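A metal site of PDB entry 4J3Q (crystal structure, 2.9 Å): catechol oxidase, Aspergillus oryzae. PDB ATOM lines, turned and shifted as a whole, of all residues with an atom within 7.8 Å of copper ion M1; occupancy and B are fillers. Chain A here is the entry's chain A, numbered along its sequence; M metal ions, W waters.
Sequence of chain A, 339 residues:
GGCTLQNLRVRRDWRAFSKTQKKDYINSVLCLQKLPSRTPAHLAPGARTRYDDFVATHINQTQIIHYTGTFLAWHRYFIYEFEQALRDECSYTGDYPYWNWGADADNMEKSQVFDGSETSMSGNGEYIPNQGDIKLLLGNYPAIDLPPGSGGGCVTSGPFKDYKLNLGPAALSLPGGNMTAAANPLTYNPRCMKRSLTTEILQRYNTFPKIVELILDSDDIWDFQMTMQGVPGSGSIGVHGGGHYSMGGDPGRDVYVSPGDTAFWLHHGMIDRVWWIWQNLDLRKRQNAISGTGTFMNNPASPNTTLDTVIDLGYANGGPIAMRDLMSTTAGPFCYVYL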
ATOM      1  N   HIS A  58     -25.511  19.435  -5.017  1.00  0.00           N
ATOM      2  CA  HIS A  58     -24.055  19.434  -4.814  1.00  0.00           C
ATOM      3  C   HIS A  58     -23.476  18.025  -4.987  1.00  0.00           C
ATOM      4  O   HIS A  58     -22.483  17.838  -5.693  1.00  0.00           O
ATOM      5  CB  HIS A  58     -23.700  19.987  -3.441  1.00  0.00           C
ATOM      6  CG  HIS A  58     -22.255  20.353  -3.277  1.00  0.00           C
ATOM      7  ND1 HIS A  58     -21.316  19.472  -2.770  1.00  0.00           N
ATOM      8  CD2 HIS A  58     -21.597  21.503  -3.520  1.00  0.00           C
ATOM      9  CE1 HIS A  58     -20.138  20.067  -2.742  1.00  0.00           C
ATOM     10  NE2 HIS A  58     -20.290  21.303  -3.185  1.00  0.00           N
ATOM     11  N   HIS A  66     -15.716  20.875  -9.105  1.00  0.00           N
ATOM     12  CA  HIS A  66     -14.526  21.055  -8.321  1.00  0.00           C
ATOM     13  C   HIS A  66     -13.384  20.684  -9.256  1.00  0.00           C
ATOM     14  O   HIS A  66     -13.496  19.689  -9.958  1.00  0.00           O
ATOM     15  CB  HIS A  66     -14.563  20.175  -7.056  1.00  0.00           C
ATOM     16  CG  HIS A  66     -15.691  20.504  -6.116  1.00  0.00           C
ATOM     17  ND1 HIS A  66     -16.811  19.721  -6.009  1.00  0.00           N
ATOM     18  CD2 HIS A  66     -15.866  21.528  -5.236  1.00  0.00           C
ATOM     19  CE1 HIS A  66     -17.633  20.242  -5.103  1.00  0.00           C
ATOM     20  NE2 HIS A  66     -17.085  21.356  -4.623  1.00  0.00           N
ATOM     21  N   PHE A  71     -15.700  26.064 -11.248  1.00  0.00           N
ATOM     22  CA  PHE A  71     -15.678  25.940  -9.786  1.00  0.00           C
ATOM     23  C   PHE A  71     -16.056  27.218  -9.085  1.00  0.00           C
ATOM     24  O   PHE A  71     -17.016  27.242  -8.326  1.00  0.00           O
ATOM     25  CB  PHE A  71     -14.299  25.443  -9.306  1.00  0.00           C
ATOM     26  CG  PHE A  71     -14.002  25.654  -7.845  1.00  0.00           C
ATOM     27  CD1 PHE A  71     -14.677  24.953  -6.873  1.00  0.00           C
ATOM     28  CD2 PHE A  71     -12.975  26.517  -7.463  1.00  0.00           C
ATOM     29  CE1 PHE A  71     -14.374  25.120  -5.528  1.00  0.00           C
ATOM     30  CE2 PHE A  71     -12.658  26.692  -6.100  1.00  0.00           C
ATOM     31  CZ  PHE A  71     -13.367  25.987  -5.136  1.00  0.00           C
ATOM     32  N   HIS A  75     -19.942  27.938  -7.665  1.00  0.00           N
ATOM     33  CA  HIS A  75     -20.160  28.208  -6.247  1.00  0.00           C
ATOM     34  C   HIS A  75     -20.694  29.596  -5.932  1.00  0.00           C
ATOM     35  O   HIS A  75     -21.440  29.784  -4.960  1.00  0.00           O
ATOM     36  CB  HIS A  75     -18.884  27.915  -5.452  1.00  0.00           C
ATOM     37  CG  HIS A  75     -18.690  26.445  -5.238  1.00  0.00           C
ATOM     38  ND1 HIS A  75     -17.974  25.657  -6.106  1.00  0.00           N
ATOM     39  CD2 HIS A  75     -19.237  25.613  -4.324  1.00  0.00           C
ATOM     40  CE1 HIS A  75     -18.034  24.395  -5.690  1.00  0.00           C
ATOM     41  NE2 HIS A  75     -18.803  24.355  -4.627  1.00  0.00           N
ATOM     42  N   HIS A 240      -9.460  26.508   0.542  1.00  0.00           N
ATOM     43  CA  HIS A 240     -10.737  25.835   0.355  1.00  0.00           C
ATOM     44  C   HIS A 240     -10.814  24.465   1.039  1.00  0.00           C
ATOM     45  O   HIS A 240     -11.840  24.105   1.607  1.00  0.00           O
ATOM     46  CB  HIS A 240     -11.070  25.713  -1.133  1.00  0.00           C
ATOM     47  CG  HIS A 240     -12.308  24.916  -1.406  1.00  0.00           C
ATOM     48  ND1 HIS A 240     -12.262  23.619  -1.878  1.00  0.00           N
ATOM     49  CD2 HIS A 240     -13.614  25.195  -1.202  1.00  0.00           C
ATOM     50  CE1 HIS A 240     -13.493  23.151  -1.984  1.00  0.00           C
ATOM     51  NE2 HIS A 240     -14.335  24.089  -1.571  1.00  0.00           N
ATOM     52  N   GLY A 241      -9.732  23.691   1.008  1.00  0.00           N
ATOM     53  CA  GLY A 241      -9.694  22.400   1.676  1.00  0.00           C
ATOM     54  C   GLY A 241      -9.534  22.572   3.184  1.00  0.00           C
ATOM     55  O   GLY A 241     -10.194  21.913   3.982  1.00  0.00           O
ATOM     56  N   GLY A 243     -10.566  24.916   5.029  1.00  0.00           N
ATOM     57  CA  GLY A 243     -11.823  25.362   5.607  1.00  0.00           C
ATOM     58  C   GLY A 243     -12.771  24.212   5.773  1.00  0.00           C
ATOM     59  O   GLY A 243     -13.493  24.133   6.783  1.00  0.00           O
ATOM     60  N   HIS A 244     -12.769  23.306   4.810  1.00  0.00           N
ATOM     61  CA  HIS A 244     -13.676  22.172   4.919  1.00  0.00           C
ATOM     62  C   HIS A 244     -13.218  21.190   5.976  1.00  0.00           C
ATOM     63  O   HIS A 244     -13.977  20.851   6.884  1.00  0.00           O
ATOM     64  CB  HIS A 244     -13.898  21.486   3.563  1.00  0.00           C
ATOM     65  CG  HIS A 244     -14.914  22.174   2.710  1.00  0.00           C
ATOM     66  ND1 HIS A 244     -16.176  22.491   3.164  1.00  0.00           N
ATOM     67  CD2 HIS A 244     -14.844  22.624   1.433  1.00  0.00           C
ATOM     68  CE1 HIS A 244     -16.843  23.103   2.206  1.00  0.00           C
ATOM     69  NE2 HIS A 244     -16.066  23.189   1.141  1.00  0.00           N
ATOM     70  N   MET A 247     -13.452  21.577   9.919  1.00  0.00           N
ATOM     71  CA  MET A 247     -14.698  21.254  10.581  1.00  0.00           C
ATOM     72  C   MET A 247     -14.777  19.754  10.994  1.00  0.00           C
ATOM     73  O   MET A 247     -15.559  19.381  11.868  1.00  0.00           O
ATOM     74  CB  MET A 247     -15.875  21.610   9.682  1.00  0.00           C
ATOM     75  CG  MET A 247     -15.812  22.988   9.152  1.00  0.00           C
ATOM     76  SD  MET A 247     -17.270  23.321   8.154  1.00  0.00           S
ATOM     77  CE  MET A 247     -16.564  24.415   6.907  1.00  0.00           C
ATOM     78  N   VAL A 255     -16.447  15.575   0.367  1.00  0.00           N
ATOM     79  CA  VAL A 255     -16.453  16.514  -0.751  1.00  0.00           C
ATOM     80  C   VAL A 255     -17.848  16.723  -1.394  1.00  0.00           C
ATOM     81  O   VAL A 255     -18.128  17.822  -1.877  1.00  0.00           O
ATOM     82  CB  VAL A 255     -15.455  16.085  -1.864  1.00  0.00           C
ATOM     83  CG1 VAL A 255     -15.496  17.056  -3.026  1.00  0.00           C
ATOM     84  CG2 VAL A 255     -14.033  15.970  -1.319  1.00  0.00           C
ATOM     85  N   SER A 258     -20.720  18.196   1.598  1.00  0.00           N
ATOM     86  CA  SER A 258     -20.240  19.333   2.405  1.00  0.00           C
ATOM     87  C   SER A 258     -21.242  20.465   2.739  1.00  0.00           C
ATOM     88  O   SER A 258     -21.205  21.002   3.852  1.00  0.00           O
ATOM     89  CB  SER A 258     -18.931  19.899   1.874  1.00  0.00           C
ATOM     90  OG  SER A 258     -19.039  20.253   0.513  1.00  0.00           O
ATOM     91  N   PRO A 259     -22.142  20.814   1.809  1.00  0.00           N
ATOM     92  CA  PRO A 259     -23.246  21.717   2.167  1.00  0.00           C
ATOM     93  C   PRO A 259     -24.110  21.225   3.337  1.00  0.00           C
ATOM     94  O   PRO A 259     -24.906  21.975   3.879  1.00  0.00           O
ATOM     95  CB  PRO A 259     -24.079  21.766   0.899  1.00  0.00           C
ATOM     96  CG  PRO A 259     -23.117  21.569  -0.157  1.00  0.00           C
ATOM     97  CD  PRO A 259     -22.116  20.591   0.352  1.00  0.00           C
ATOM     98  N   PHE A 264     -20.868  25.668   5.665  1.00  0.00           N
ATOM     99  CA  PHE A 264     -20.523  25.678   4.247  1.00  0.00           C
ATOM    100  C   PHE A 264     -20.673  27.064   3.620  1.00  0.00           C
ATOM    101  O   PHE A 264     -19.747  27.572   3.013  1.00  0.00           O
ATOM    102  CB  PHE A 264     -21.399  24.714   3.490  1.00  0.00           C
ATOM    103  CG  PHE A 264     -21.175  24.718   2.000  1.00  0.00           C
ATOM    104  CD1 PHE A 264     -21.955  25.491   1.170  1.00  0.00           C
ATOM    105  CD2 PHE A 264     -20.213  23.897   1.433  1.00  0.00           C
ATOM    106  CE1 PHE A 264     -21.773  25.453  -0.191  1.00  0.00           C
ATOM    107  CE2 PHE A 264     -20.027  23.856   0.081  1.00  0.00           C
ATOM    108  CZ  PHE A 264     -20.812  24.625  -0.736  1.00  0.00           C
ATOM    109  N   HIS A 267     -18.315  29.556   4.884  1.00  0.00           N
ATOM    110  CA  HIS A 267     -17.040  29.224   4.297  1.00  0.00           C
ATOM    111  C   HIS A 267     -16.949  29.754   2.865  1.00  0.00           C
ATOM    112  O   HIS A 267     -15.995  30.442   2.521  1.00  0.00           O
ATOM    113  CB  HIS A 267     -16.781  27.705   4.344  1.00  0.00           C
ATOM    114  CG  HIS A 267     -15.545  27.265   3.620  1.00  0.00           C
ATOM    115  ND1 HIS A 267     -14.328  27.893   3.753  1.00  0.00           N
ATOM    116  CD2 HIS A 267     -15.343  26.241   2.751  1.00  0.00           C
ATOM    117  CE1 HIS A 267     -13.440  27.288   2.998  1.00  0.00           C
ATOM    118  NE2 HIS A 267     -14.026  26.282   2.374  1.00  0.00           N
ATOM    119  N   HIS A 268     -17.949  29.454   2.054  1.00  0.00           N
ATOM    120  CA  HIS A 268     -17.894  29.822   0.638  1.00  0.00           C
ATOM    121  C   HIS A 268     -18.139  31.309   0.384  1.00  0.00           C
ATOM    122  O   HIS A 268     -17.852  31.804  -0.704  1.00  0.00           O
ATOM    123  CB  HIS A 268     -18.847  28.975  -0.211  1.00  0.00           C
ATOM    124  CG  HIS A 268     -18.224  27.733  -0.749  1.00  0.00           C
ATOM    125  ND1 HIS A 268     -17.500  27.719  -1.921  1.00  0.00           N
ATOM    126  CD2 HIS A 268     -18.195  26.465  -0.273  1.00  0.00           C
ATOM    127  CE1 HIS A 268     -17.044  26.496  -2.134  1.00  0.00           C
ATOM    128  NE2 HIS A 268     -17.473  25.715  -1.154  1.00  0.00           N
ATOM    129  N   ILE A 271     -14.653  32.329   0.265  1.00  0.00           N
ATOM    130  CA  ILE A 271     -14.062  31.906  -0.998  1.00  0.00           C
ATOM    131  C   ILE A 271     -14.398  32.945  -2.035  1.00  0.00           C
ATOM    132  O   ILE A 271     -13.573  33.400  -2.815  1.00  0.00           O
ATOM    133  CB  ILE A 271     -14.599  30.476  -1.458  1.00  0.00           C
ATOM    134  CG1 ILE A 271     -14.142  29.361  -0.483  1.00  0.00           C
ATOM    135  CG2 ILE A 271     -14.192  30.145  -2.919  1.00  0.00           C
ATOM    136  CD1 ILE A 271     -12.605  29.127  -0.492  1.00  0.00           C
HETATM  137 CU    CU M   1     -16.219  24.143  -0.697  1.00  0.00          CU
HETATM  138 CU    CU M   2     -18.718  22.481  -3.838  1.00  0.00          CU
HETATM  139  O   HOH W   1     -17.193  22.283  -1.910  1.00  0.00           O
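A ring nitrogen (NE2) of His 267 lies within hydrogen-bond range of the backbone carbonyl oxygen of His 240, at 3.2 Å.
Merely in contact with copper ion M1: Phe 264.
Four residues have an atom within 4 Å of copper ion M1: His 240, His 244, Phe 264 and His 268.
Copper ion M1 is bound by NE2 of His 268 (2.1 Å), NE2 of His 244 (2.1 Å), NE2 of His 240 (2.1 Å) and water W1 (2.4 Å).
Copper ion M1 has four donor atoms within binding distance.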
